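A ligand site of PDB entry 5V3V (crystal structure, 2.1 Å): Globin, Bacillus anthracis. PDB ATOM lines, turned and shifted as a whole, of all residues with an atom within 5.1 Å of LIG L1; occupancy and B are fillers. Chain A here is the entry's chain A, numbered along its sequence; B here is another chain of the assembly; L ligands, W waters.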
ATOM      1  N   LEU A  35     -16.009 -31.339  21.805  1.00  0.00           N
ATOM      2  CA  LEU A  35     -14.791 -31.088  21.036  1.00  0.00           C
ATOM      3  C   LEU A  35     -14.561 -32.058  19.900  1.00  0.00           C
ATOM      4  O   LEU A  35     -14.130 -31.638  18.823  1.00  0.00           O
ATOM      5  CB  LEU A  35     -13.562 -31.134  21.955  1.00  0.00           C
ATOM      6  CG  LEU A  35     -13.475 -30.059  23.029  1.00  0.00           C
ATOM      7  CD1 LEU A  35     -12.202 -30.275  23.799  1.00  0.00           C
ATOM      8  CD2 LEU A  35     -13.516 -28.677  22.378  1.00  0.00           C
ATOM      9  N   ILE A  38     -15.470 -31.409  15.915  1.00  0.00           N
ATOM     10  CA  ILE A  38     -14.714 -30.480  15.085  1.00  0.00           C
ATOM     11  C   ILE A  38     -13.267 -30.912  14.880  1.00  0.00           C
ATOM     12  O   ILE A  38     -12.598 -30.376  13.984  1.00  0.00           O
ATOM     13  CB  ILE A  38     -14.770 -29.048  15.651  1.00  0.00           C
ATOM     14  CG1 ILE A  38     -14.177 -28.987  17.060  1.00  0.00           C
ATOM     15  CG2 ILE A  38     -16.205 -28.541  15.649  1.00  0.00           C
ATOM     16  CD1 ILE A  38     -15.207 -28.733  18.153  1.00  0.00           C
ATOM     17  N   PHE A  39     -12.807 -31.833  15.621  1.00  0.00           N
ATOM     18  CA  PHE A  39     -11.437 -32.275  15.340  1.00  0.00           C
ATOM     19  C   PHE A  39     -11.418 -33.407  14.331  1.00  0.00           C
ATOM     20  O   PHE A  39     -12.386 -34.178  14.230  1.00  0.00           O
ATOM     21  CB  PHE A  39     -10.772 -32.758  16.613  1.00  0.00           C
ATOM     22  CG  PHE A  39     -10.424 -31.662  17.546  1.00  0.00           C
ATOM     23  CD1 PHE A  39      -9.170 -31.119  17.536  1.00  0.00           C
ATOM     24  CD2 PHE A  39     -11.355 -31.163  18.447  1.00  0.00           C
ATOM     25  CE1 PHE A  39      -8.865 -30.120  18.392  1.00  0.00           C
ATOM     26  CE2 PHE A  39     -11.040 -30.160  19.303  1.00  0.00           C
ATOM     27  CZ  PHE A  39      -9.791 -29.634  19.279  1.00  0.00           C
ATOM     28  N   PRO A  40     -10.316 -33.532  13.558  1.00  0.00           N
ATOM     29  CA  PRO A  40     -10.161 -34.694  12.686  1.00  0.00           C
ATOM     30  C   PRO A  40     -10.381 -36.011  13.418  1.00  0.00           C
ATOM     31  O   PRO A  40     -10.241 -36.081  14.647  1.00  0.00           O
ATOM     32  CB  PRO A  40      -8.721 -34.548  12.174  1.00  0.00           C
ATOM     33  CG  PRO A  40      -8.496 -33.081  12.161  1.00  0.00           C
ATOM     34  CD  PRO A  40      -9.247 -32.541  13.362  1.00  0.00           C
ATOM     35  N   THR A  46      -2.714 -33.593  14.545  1.00  0.00           N
ATOM     36  CA  THR A  46      -3.017 -32.506  15.460  1.00  0.00           C
ATOM     37  C   THR A  46      -2.111 -32.566  16.686  1.00  0.00           C
ATOM     38  O   THR A  46      -1.491 -31.561  17.065  1.00  0.00           O
ATOM     39  CB  THR A  46      -4.491 -32.547  15.882  1.00  0.00           C
ATOM     40  OG1 THR A  46      -5.319 -32.521  14.719  1.00  0.00           O
ATOM     41  CG2 THR A  46      -4.845 -31.337  16.742  1.00  0.00           C
ATOM     42  N   LYS A  49       1.471 -31.515  15.953  1.00  0.00           N
ATOM     43  CA  LYS A  49       1.556 -30.059  15.889  1.00  0.00           C
ATOM     44  C   LYS A  49       1.412 -29.420  17.280  1.00  0.00           C
ATOM     45  O   LYS A  49       2.172 -28.504  17.620  1.00  0.00           O
ATOM     46  CB  LYS A  49       0.497 -29.523  14.903  1.00  0.00           C
ATOM     47  CG  LYS A  49       0.787 -29.846  13.442  1.00  0.00           C
ATOM     48  CD  LYS A  49      -0.232 -29.226  12.455  1.00  0.00           C
ATOM     49  CE  LYS A  49      -1.618 -29.837  12.566  1.00  0.00           C
ATOM     50  NZ  LYS A  49      -2.404 -29.747  11.275  1.00  0.00           N
ATOM     51  N   GLN A  50       0.485 -29.912  18.102  1.00  0.00           N
ATOM     52  CA  GLN A  50       0.329 -29.374  19.460  1.00  0.00           C
ATOM     53  C   GLN A  50       1.611 -29.477  20.263  1.00  0.00           C
ATOM     54  O   GLN A  50       1.992 -28.536  20.983  1.00  0.00           O
ATOM     55  CB  GLN A  50      -0.780 -30.101  20.228  1.00  0.00           C
ATOM     56  CG  GLN A  50      -2.199 -29.965  19.684  1.00  0.00           C
ATOM     57  CD  GLN A  50      -3.117 -31.078  20.191  1.00  0.00           C
ATOM     58  OE1 GLN A  50      -2.676 -32.184  20.497  1.00  0.00           O
ATOM     59  NE2 GLN A  50      -4.391 -30.795  20.269  1.00  0.00           N
ATOM     60  N   PHE A  53       3.918 -26.910  18.978  1.00  0.00           N
ATOM     61  CA  PHE A  53       3.512 -25.578  19.413  1.00  0.00           C
ATOM     62  C   PHE A  53       3.840 -25.352  20.872  1.00  0.00           C
ATOM     63  O   PHE A  53       4.473 -24.352  21.230  1.00  0.00           O
ATOM     64  CB  PHE A  53       2.008 -25.348  19.202  1.00  0.00           C
ATOM     65  CG  PHE A  53       1.582 -23.985  19.641  1.00  0.00           C
ATOM     66  CD1 PHE A  53       1.903 -22.877  18.864  1.00  0.00           C
ATOM     67  CD2 PHE A  53       0.938 -23.797  20.844  1.00  0.00           C
ATOM     68  CE1 PHE A  53       1.556 -21.604  19.276  1.00  0.00           C
ATOM     69  CE2 PHE A  53       0.581 -22.527  21.255  1.00  0.00           C
ATOM     70  CZ  PHE A  53       0.895 -21.429  20.471  1.00  0.00           C
ATOM     71  N   LEU A  54       3.387 -26.257  21.734  1.00  0.00           N
ATOM     72  CA  LEU A  54       3.558 -26.060  23.171  1.00  0.00           C
ATOM     73  C   LEU A  54       5.025 -26.036  23.549  1.00  0.00           C
ATOM     74  O   LEU A  54       5.414 -25.318  24.474  1.00  0.00           O
ATOM     75  CB  LEU A  54       2.830 -27.160  23.951  1.00  0.00           C
ATOM     76  CG  LEU A  54       1.311 -27.151  23.979  1.00  0.00           C
ATOM     77  CD1 LEU A  54       0.786 -28.356  24.788  1.00  0.00           C
ATOM     78  CD2 LEU A  54       0.776 -25.832  24.562  1.00  0.00           C
ATOM     79  N   TYR A  57       6.002 -22.586  22.662  1.00  0.00           N
ATOM     80  CA  TYR A  57       5.160 -21.707  23.466  1.00  0.00           C
ATOM     81  C   TYR A  57       5.718 -21.554  24.870  1.00  0.00           C
ATOM     82  O   TYR A  57       5.563 -20.491  25.476  1.00  0.00           O
ATOM     83  CB  TYR A  57       3.739 -22.288  23.488  1.00  0.00           C
ATOM     84  CG  TYR A  57       2.632 -21.570  24.251  1.00  0.00           C
ATOM     85  CD1 TYR A  57       1.848 -20.592  23.638  1.00  0.00           C
ATOM     86  CD2 TYR A  57       2.312 -21.944  25.553  1.00  0.00           C
ATOM     87  CE1 TYR A  57       0.791 -19.967  24.322  1.00  0.00           C
ATOM     88  CE2 TYR A  57       1.257 -21.332  26.252  1.00  0.00           C
ATOM     89  CZ  TYR A  57       0.503 -20.346  25.626  1.00  0.00           C
ATOM     90  OH  TYR A  57      -0.537 -19.746  26.312  1.00  0.00           O
ATOM     91  N   TYR A  64       7.539 -25.572  16.049  1.00  0.00           N
ATOM     92  CA  TYR A  64       6.348 -25.238  15.259  1.00  0.00           C
ATOM     93  C   TYR A  64       6.667 -24.218  14.187  1.00  0.00           C
ATOM     94  O   TYR A  64       6.423 -24.461  12.996  1.00  0.00           O
ATOM     95  CB  TYR A  64       5.225 -24.717  16.162  1.00  0.00           C
ATOM     96  CG  TYR A  64       3.954 -24.502  15.349  1.00  0.00           C
ATOM     97  CD1 TYR A  64       3.789 -23.364  14.570  1.00  0.00           C
ATOM     98  CD2 TYR A  64       2.947 -25.455  15.350  1.00  0.00           C
ATOM     99  CE1 TYR A  64       2.661 -23.189  13.817  1.00  0.00           C
ATOM    100  CE2 TYR A  64       1.804 -25.269  14.609  1.00  0.00           C
ATOM    101  CZ  TYR A  64       1.670 -24.129  13.839  1.00  0.00           C
ATOM    102  OH  TYR A  64       0.537 -23.940  13.099  1.00  0.00           O
ATOM    103  N   HIS A  68       6.024 -24.883  10.354  1.00  0.00           N
ATOM    104  CA  HIS A  68       4.731 -24.455   9.846  1.00  0.00           C
ATOM    105  C   HIS A  68       4.617 -22.957   9.599  1.00  0.00           C
ATOM    106  O   HIS A  68       3.612 -22.512   9.051  1.00  0.00           O
ATOM    107  CB  HIS A  68       3.632 -24.877  10.818  1.00  0.00           C
ATOM    108  CG  HIS A  68       3.710 -26.311  11.224  1.00  0.00           C
ATOM    109  ND1 HIS A  68       3.086 -27.316  10.534  1.00  0.00           N
ATOM    110  CD2 HIS A  68       4.349 -26.915  12.258  1.00  0.00           C
ATOM    111  CE1 HIS A  68       3.328 -28.472  11.119  1.00  0.00           C
ATOM    112  NE2 HIS A  68       4.096 -28.255  12.159  1.00  0.00           N
ATOM    113  N   LEU A  73      -2.476 -18.253  15.699  1.00  0.00           N
ATOM    114  CA  LEU A  73      -3.456 -19.263  16.065  1.00  0.00           C
ATOM    115  C   LEU A  73      -4.870 -18.733  15.957  1.00  0.00           C
ATOM    116  O   LEU A  73      -5.785 -19.501  15.619  1.00  0.00           O
ATOM    117  CB  LEU A  73      -3.194 -19.775  17.484  1.00  0.00           C
ATOM    118  CG  LEU A  73      -2.027 -20.718  17.730  1.00  0.00           C
ATOM    119  CD1 LEU A  73      -2.181 -21.373  19.099  1.00  0.00           C
ATOM    120  CD2 LEU A  73      -1.943 -21.769  16.645  1.00  0.00           C
ATOM    121  N   ARG A  76      -5.529 -19.195  12.352  1.00  0.00           N
ATOM    122  CA  ARG A  76      -5.686 -20.609  12.006  1.00  0.00           C
ATOM    123  C   ARG A  76      -6.958 -21.228  12.548  1.00  0.00           C
ATOM    124  O   ARG A  76      -7.369 -22.291  12.064  1.00  0.00           O
ATOM    125  CB  ARG A  76      -4.506 -21.419  12.504  1.00  0.00           C
ATOM    126  CG  ARG A  76      -3.177 -20.975  11.955  1.00  0.00           C
ATOM    127  CD  ARG A  76      -2.180 -22.083  12.153  1.00  0.00           C
ATOM    128  NE  ARG A  76      -0.815 -21.668  11.870  1.00  0.00           N
ATOM    129  CZ  ARG A  76      -0.100 -22.108  10.834  1.00  0.00           C
ATOM    130  NH1 ARG A  76       1.144 -21.691  10.671  1.00  0.00           N
ATOM    131  NH2 ARG A  76      -0.641 -22.966   9.975  1.00  0.00           N
ATOM    132  N   HIS A  77      -7.593 -20.615  13.549  1.00  0.00           N
ATOM    133  CA  HIS A  77      -8.825 -21.150  14.091  1.00  0.00           C
ATOM    134  C   HIS A  77     -10.060 -20.437  13.557  1.00  0.00           C
ATOM    135  O   HIS A  77     -11.171 -20.747  13.994  1.00  0.00           O
ATOM    136  CB  HIS A  77      -8.800 -21.083  15.629  1.00  0.00           C
ATOM    137  CG  HIS A  77      -7.887 -22.084  16.265  1.00  0.00           C
ATOM    138  ND1 HIS A  77      -6.515 -21.910  16.307  1.00  0.00           N
ATOM    139  CD2 HIS A  77      -8.129 -23.259  16.871  1.00  0.00           C
ATOM    140  CE1 HIS A  77      -5.967 -22.938  16.922  1.00  0.00           C
ATOM    141  NE2 HIS A  77      -6.921 -23.773  17.277  1.00  0.00           N
ATOM    142  N   PHE A  80     -13.132 -22.602  12.347  1.00  0.00           N
ATOM    143  CA  PHE A  80     -13.654 -23.573  13.285  1.00  0.00           C
ATOM    144  C   PHE A  80     -14.600 -22.920  14.272  1.00  0.00           C
ATOM    145  O   PHE A  80     -14.369 -21.803  14.744  1.00  0.00           O
ATOM    146  CB  PHE A  80     -12.500 -24.256  14.011  1.00  0.00           C
ATOM    147  CG  PHE A  80     -11.454 -24.792  13.083  1.00  0.00           C
ATOM    148  CD1 PHE A  80     -11.841 -25.518  11.960  1.00  0.00           C
ATOM    149  CD2 PHE A  80     -10.112 -24.545  13.307  1.00  0.00           C
ATOM    150  CE1 PHE A  80     -10.882 -26.009  11.075  1.00  0.00           C
ATOM    151  CE2 PHE A  80      -9.156 -25.023  12.421  1.00  0.00           C
ATOM    152  CZ  PHE A  80      -9.541 -25.755  11.306  1.00  0.00           C
ATOM    153  N   ILE A  82     -15.504 -22.110  17.377  1.00  0.00           N
ATOM    154  CA  ILE A  82     -14.931 -22.073  18.714  1.00  0.00           C
ATOM    155  C   ILE A  82     -15.789 -21.145  19.565  1.00  0.00           C
ATOM    156  O   ILE A  82     -15.644 -19.920  19.540  1.00  0.00           O
ATOM    157  CB  ILE A  82     -13.469 -21.649  18.706  1.00  0.00           C
ATOM    158  CG1 ILE A  82     -12.669 -22.630  17.847  1.00  0.00           C
ATOM    159  CG2 ILE A  82     -12.925 -21.638  20.135  1.00  0.00           C
ATOM    160  CD1 ILE A  82     -11.217 -22.411  17.914  1.00  0.00           C
ATOM    161  N   ARG A  86     -16.733 -24.316  24.082  1.00  0.00           N
ATOM    162  CA  ARG A  86     -15.698 -25.208  23.610  1.00  0.00           C
ATOM    163  C   ARG A  86     -14.331 -24.802  24.135  1.00  0.00           C
ATOM    164  O   ARG A  86     -13.477 -25.667  24.402  1.00  0.00           O
ATOM    165  CB  ARG A  86     -15.711 -25.279  22.080  1.00  0.00           C
ATOM    166  CG  ARG A  86     -16.906 -26.056  21.583  1.00  0.00           C
ATOM    167  CD  ARG A  86     -16.973 -26.083  20.063  1.00  0.00           C
ATOM    168  NE  ARG A  86     -17.787 -27.196  19.584  1.00  0.00           N
ATOM    169  CZ  ARG A  86     -18.445 -27.219  18.425  1.00  0.00           C
ATOM    170  NH1 ARG A  86     -18.409 -26.167  17.625  1.00  0.00           N
ATOM    171  NH2 ARG A  86     -19.153 -28.290  18.086  1.00  0.00           N
ATOM    172  N   ALA A  87     -14.116 -23.496  24.331  1.00  0.00           N
ATOM    173  CA  ALA A  87     -12.901 -23.058  25.009  1.00  0.00           C
ATOM    174  C   ALA A  87     -12.833 -23.622  26.418  1.00  0.00           C
ATOM    175  O   ALA A  87     -11.773 -24.095  26.850  1.00  0.00           O
ATOM    176  CB  ALA A  87     -12.818 -21.533  25.007  1.00  0.00           C
ATOM    177  N   TRP A  90     -12.002 -27.267  26.116  1.00  0.00           N
ATOM    178  CA  TRP A  90     -10.575 -27.343  25.829  1.00  0.00           C
ATOM    179  C   TRP A  90      -9.736 -27.280  27.097  1.00  0.00           C
ATOM    180  O   TRP A  90      -8.910 -28.159  27.370  1.00  0.00           O
ATOM    181  CB  TRP A  90     -10.172 -26.204  24.915  1.00  0.00           C
ATOM    182  CG  TRP A  90      -8.889 -26.407  24.254  1.00  0.00           C
ATOM    183  CD1 TRP A  90      -8.716 -26.877  23.009  1.00  0.00           C
ATOM    184  CD2 TRP A  90      -7.566 -26.145  24.781  1.00  0.00           C
ATOM    185  NE1 TRP A  90      -7.372 -26.953  22.724  1.00  0.00           N
ATOM    186  CE2 TRP A  90      -6.641 -26.489  23.776  1.00  0.00           C
ATOM    187  CE3 TRP A  90      -7.080 -25.652  26.001  1.00  0.00           C
ATOM    188  CZ2 TRP A  90      -5.265 -26.353  23.934  1.00  0.00           C
ATOM    189  CZ3 TRP A  90      -5.689 -25.533  26.167  1.00  0.00           C
ATOM    190  CH2 TRP A  90      -4.813 -25.885  25.139  1.00  0.00           C
ATOM    191  N   LEU A 115      -2.354 -20.585  28.868  1.00  0.00           N
ATOM    192  CA  LEU A 115      -3.202 -21.331  27.952  1.00  0.00           C
ATOM    193  C   LEU A 115      -4.648 -20.832  27.999  1.00  0.00           C
ATOM    194  O   LEU A 115      -5.331 -20.790  26.971  1.00  0.00           O
ATOM    195  CB  LEU A 115      -3.127 -22.814  28.274  1.00  0.00           C
ATOM    196  CG  LEU A 115      -1.826 -23.514  27.883  1.00  0.00           C
ATOM    197  CD1 LEU A 115      -1.847 -24.937  28.332  1.00  0.00           C
ATOM    198  CD2 LEU A 115      -1.654 -23.475  26.390  1.00  0.00           C
ATOM    199  N   THR A 118      -4.872 -17.817  25.754  1.00  0.00           N
ATOM    200  CA  THR A 118      -4.901 -18.195  24.346  1.00  0.00           C
ATOM    201  C   THR A 118      -6.260 -18.770  23.953  1.00  0.00           C
ATOM    202  O   THR A 118      -6.791 -18.440  22.884  1.00  0.00           O
ATOM    203  CB  THR A 118      -3.788 -19.220  24.066  1.00  0.00           C
ATOM    204  OG1 THR A 118      -2.557 -18.739  24.602  1.00  0.00           O
ATOM    205  CG2 THR A 118      -3.620 -19.468  22.559  1.00  0.00           C
ATOM    206  N   ALA A 119      -6.837 -19.636  24.793  1.00  0.00           N
ATOM    207  CA  ALA A 119      -8.145 -20.228  24.510  1.00  0.00           C
ATOM    208  C   ALA A 119      -9.205 -19.153  24.310  1.00  0.00           C
ATOM    209  O   ALA A 119      -9.931 -19.151  23.309  1.00  0.00           O
ATOM    210  CB  ALA A 119      -8.545 -21.188  25.639  1.00  0.00           C
ATOM    211  N   MET A 122      -9.064 -17.673  21.102  1.00  0.00           N
ATOM    212  CA  MET A 122      -9.492 -18.469  19.950  1.00  0.00           C
ATOM    213  C   MET A 122     -10.993 -18.357  19.700  1.00  0.00           C
ATOM    214  O   MET A 122     -11.423 -18.538  18.560  1.00  0.00           O
ATOM    215  CB  MET A 122      -9.100 -19.946  20.136  1.00  0.00           C
ATOM    216  CG  MET A 122      -7.609 -20.233  20.312  1.00  0.00           C
ATOM    217  SD  MET A 122      -6.579 -19.671  18.934  1.00  0.00           S
ATOM    218  CE  MET A 122      -6.055 -18.046  19.509  1.00  0.00           C
ATOM    219  N   ARG B 114      -7.048 -27.862   4.457  1.00  0.00           N
ATOM    220  CA  ARG B 114      -7.723 -27.068   5.478  1.00  0.00           C
ATOM    221  C   ARG B 114      -9.099 -26.610   4.999  1.00  0.00           C
ATOM    222  O   ARG B 114     -10.045 -26.530   5.797  1.00  0.00           O
ATOM    223  CB  ARG B 114      -6.846 -25.869   5.874  1.00  0.00           C
ATOM    224  CG  ARG B 114      -5.698 -26.296   6.777  1.00  0.00           C
ATOM    225  CD  ARG B 114      -4.473 -25.430   6.629  1.00  0.00           C
ATOM    226  NE  ARG B 114      -3.501 -25.805   7.641  1.00  0.00           N
ATOM    227  CZ  ARG B 114      -2.725 -26.889   7.562  1.00  0.00           C
ATOM    228  NH1 ARG B 114      -2.804 -27.690   6.502  1.00  0.00           N
ATOM    229  NH2 ARG B 114      -1.859 -27.170   8.529  1.00  0.00           N
ATOM    230  N   LEU B 117     -11.372 -29.699   5.210  1.00  0.00           N
ATOM    231  CA  LEU B 117     -11.826 -29.863   6.590  1.00  0.00           C
ATOM    232  C   LEU B 117     -12.885 -28.822   6.929  1.00  0.00           C
ATOM    233  O   LEU B 117     -13.918 -29.147   7.527  1.00  0.00           O
ATOM    234  CB  LEU B 117     -10.658 -29.769   7.565  1.00  0.00           C
ATOM    235  CG  LEU B 117     -11.108 -29.928   9.030  1.00  0.00           C
ATOM    236  CD1 LEU B 117     -11.551 -31.375   9.349  1.00  0.00           C
ATOM    237  CD2 LEU B 117     -10.074 -29.465  10.051  1.00  0.00           C
ATOM    238  N   HIS B 121     -16.973 -29.071   8.006  1.00  0.00           N
ATOM    239  CA  HIS B 121     -17.594 -28.468   9.185  1.00  0.00           C
ATOM    240  C   HIS B 121     -18.844 -27.661   8.846  1.00  0.00           C
ATOM    241  O   HIS B 121     -19.729 -27.511   9.695  1.00  0.00           O
ATOM    242  CB  HIS B 121     -16.567 -27.579   9.910  1.00  0.00           C
ATOM    243  CG  HIS B 121     -15.535 -28.353  10.660  1.00  0.00           C
ATOM    244  ND1 HIS B 121     -15.503 -29.730  10.665  1.00  0.00           N
ATOM    245  CD2 HIS B 121     -14.494 -27.943  11.428  1.00  0.00           C
ATOM    246  CE1 HIS B 121     -14.485 -30.148  11.411  1.00  0.00           C
ATOM    247  NE2 HIS B 121     -13.868 -29.074  11.880  1.00  0.00           N
HETATM  248  C1  LIG L   1      -5.694 -26.595  15.276  1.00  0.00           C
HETATM  249  C2  LIG L   1      -9.833 -26.583  17.916  1.00  0.00           C
HETATM  250  C3  LIG L   1      -7.609 -23.732  21.238  1.00  0.00           C
HETATM  251  C4  LIG L   1      -3.252 -24.615  19.132  1.00  0.00           C
HETATM  252  C5  LIG L   1      -7.011 -26.830  15.670  1.00  0.00           C
HETATM  253  C6  LIG L   1      -8.064 -27.506  14.923  1.00  0.00           C
HETATM  254  C7  LIG L   1      -9.185 -27.497  15.663  1.00  0.00           C
HETATM  255  C8  LIG L   1      -8.910 -26.804  16.901  1.00  0.00           C
HETATM  256  C9  LIG L   1     -10.569 -28.092  15.284  1.00  0.00           C
HETATM  257  C10 LIG L   1      -7.904 -28.162  13.527  1.00  0.00           C
HETATM  258  C11 LIG L   1      -6.947 -29.348  13.689  1.00  0.00           C
HETATM  259  C12 LIG L   1      -6.057 -29.484  12.471  1.00  0.00           C
HETATM  260  O1  LIG L   1      -6.454 -28.994  11.384  1.00  0.00           O
HETATM  261  O2  LIG L   1      -4.962 -30.100  12.604  1.00  0.00           O
HETATM  262  C13 LIG L   1      -9.577 -25.791  19.015  1.00  0.00           C
HETATM  263  C14 LIG L   1     -10.568 -25.392  19.985  1.00  0.00           C
HETATM  264  C15 LIG L   1      -9.973 -24.590  20.892  1.00  0.00           C
HETATM  265  C16 LIG L   1      -8.568 -24.461  20.549  1.00  0.00           C
HETATM  266  C17 LIG L   1     -12.048 -25.815  19.943  1.00  0.00           C
HETATM  267  C18 LIG L   1     -10.670 -23.941  22.100  1.00  0.00           C
HETATM  268  C19 LIG L   1     -10.307 -22.725  22.514  1.00  0.00           C
HETATM  269  C20 LIG L   1      -6.243 -23.834  21.048  1.00  0.00           C
HETATM  270  C21 LIG L   1      -5.192 -23.458  21.987  1.00  0.00           C
HETATM  271  C22 LIG L   1      -4.010 -23.716  21.378  1.00  0.00           C
HETATM  272  C23 LIG L   1      -4.249 -24.257  20.053  1.00  0.00           C
HETATM  273  C24 LIG L   1      -5.468 -22.869  23.399  1.00  0.00           C
HETATM  274  C25 LIG L   1      -2.574 -23.525  21.899  1.00  0.00           C
HETATM  275  C26 LIG L   1      -2.306 -23.236  23.169  1.00  0.00           C
HETATM  276  C27 LIG L   1      -3.553 -25.212  17.890  1.00  0.00           C
HETATM  277  C28 LIG L   1      -2.598 -25.580  16.845  1.00  0.00           C
HETATM  278  C29 LIG L   1      -3.261 -26.106  15.806  1.00  0.00           C
HETATM  279  C30 LIG L   1      -4.684 -26.124  16.117  1.00  0.00           C
HETATM  280  C31 LIG L   1      -1.064 -25.398  16.919  1.00  0.00           C
HETATM  281  C32 LIG L   1      -2.625 -26.629  14.506  1.00  0.00           C
HETATM  282  C33 LIG L   1      -2.735 -25.555  13.428  1.00  0.00           C
HETATM  283  C34 LIG L   1      -2.032 -26.029  12.187  1.00  0.00           C
HETATM  284  O3  LIG L   1      -2.714 -26.504  11.251  1.00  0.00           O
HETATM  285  O4  LIG L   1      -0.780 -25.928  12.132  1.00  0.00           O
HETATM  286  N1  LIG L   1      -7.583 -26.411  16.864  1.00  0.00           N
HETATM  287  N2  LIG L   1      -8.376 -25.208  19.390  1.00  0.00           N
HETATM  288  N3  LIG L   1      -5.625 -24.319  19.894  1.00  0.00           N
HETATM  289  N4  LIG L   1      -4.814 -25.553  17.391  1.00  0.00           N
HETATM  290 FE1  LIG L   1      -6.602 -25.470  18.393  1.00  0.00          FE
HETATM  291  C1  LG2 L   2      -6.058 -27.331  19.250  1.00  0.00           C
HETATM  292  N1  LG2 L   2      -6.071 -28.257  19.941  1.00  0.00           N
HETATM  293  O   HOH W   1      -5.360 -26.501  11.041  1.00  0.00           O
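Ile 38 touches LIG L1 (O to C9, 3.3 Å). Phe 39 touches LIG L1. Pro 40 touches LIG L1. CE2 of Phe 53 touches C25 of LIG L1, at 3.4 Å. CD1 of Leu 73 touches C4 of LIG L1 (3.4 Å). Phe 80 touches LIG L1 (CE2 to C10, 3.6 Å). CD1 of Ile 82 touches C14 of LIG L1 (3.7 Å). Ala 87 touches LIG L1. Trp 90 touches LIG L1 (CD1 to C15, 3.4 Å). CD2 of Leu 115 touches C26 of LIG L1, 3.3 Å away. Thr 118 touches LIG L1. Ala 119 touches LIG L1 (O to C19, 3.7 Å). CG of Met 122 touches C3 of LIG L1 (3.6 Å). Leu 117 of chain B touches LIG L1. Hydrophobic or aromatic side chains within 4 Å of LIG L1: Phe 39, Pro 40, Phe 53, Tyr 64, Leu 73, His 77, Phe 80, Ile 82, Ala 87, Trp 90, Leu 115, Ala 119, Met 122 and Leu 117 of chain B. 20 residues have an atom within 4 Å of LIG L1: Ile 38, Phe 39, Pro 40, Thr 46, Lys 49, Phe 53, Tyr 64, Leu 73, Arg 76, His 77, Phe 80, Ile 82, Ala 87, Trp 90, Leu 115, Thr 118, Ala 119, Met 122, Arg 114 of chain B and Leu 117 of chain B.
A ring nitrogen (ND1) of His 77 is in hydrogen-bond range of the backbone carbonyl oxygen (O) of Leu 73 (2.6 Å). ND1 of His 77 lies within hydrogen-bond range of SD of Met 122 (3.5 Å). OH of Tyr 64 sits at hydrogen-bond distance from NE of Arg 76 (2.9 Å). N of Leu 115 lies within hydrogen-bond range of OH of Tyr 57 (3.2 Å). O of Ile 38 is in hydrogen-bond range of NE2 of His 121 of chain B. The guanidinium group (NH1) of Arg 76 sits at hydrogen-bond distance from the backbone carbonyl oxygen (O) of His 68. OG1 of Thr 118 is in hydrogen-bond range of OH of Tyr 57, at 2.8 Å.
FE1 of LIG L1 is bound by NE2 of His 77, 2.1 Å away. The side-chain hydroxyl of Tyr 64 is in hydrogen-bond range of an oxygen (O4) of LIG L1, at 2.6 Å. O2 of LIG L1 is in salt-bridge range of NZ of Lys 49, at 2.9 Å. The guanidinium group of Arg 114 of chain B is in salt-bridge range of an oxygen (O3) of LIG L1 (2.9 Å). OG1 of Thr 46 is in hydrogen-bond range of O2 of LIG L1, at 3.2 Å. NH2 of Arg 76 lies within salt-bridge range of O4 of LIG L1, 3.7 Å away. The indole nitrogen (NE1) of Trp 90 is in hydrogen-bond range of a nitrogen (N1) of LG2 L2, 3.3 Å away. A nitrogen (N1) of LG2 L2 sits at hydrogen-bond distance from the side-chain amide nitrogen of Gln 50 (3.1 Å).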
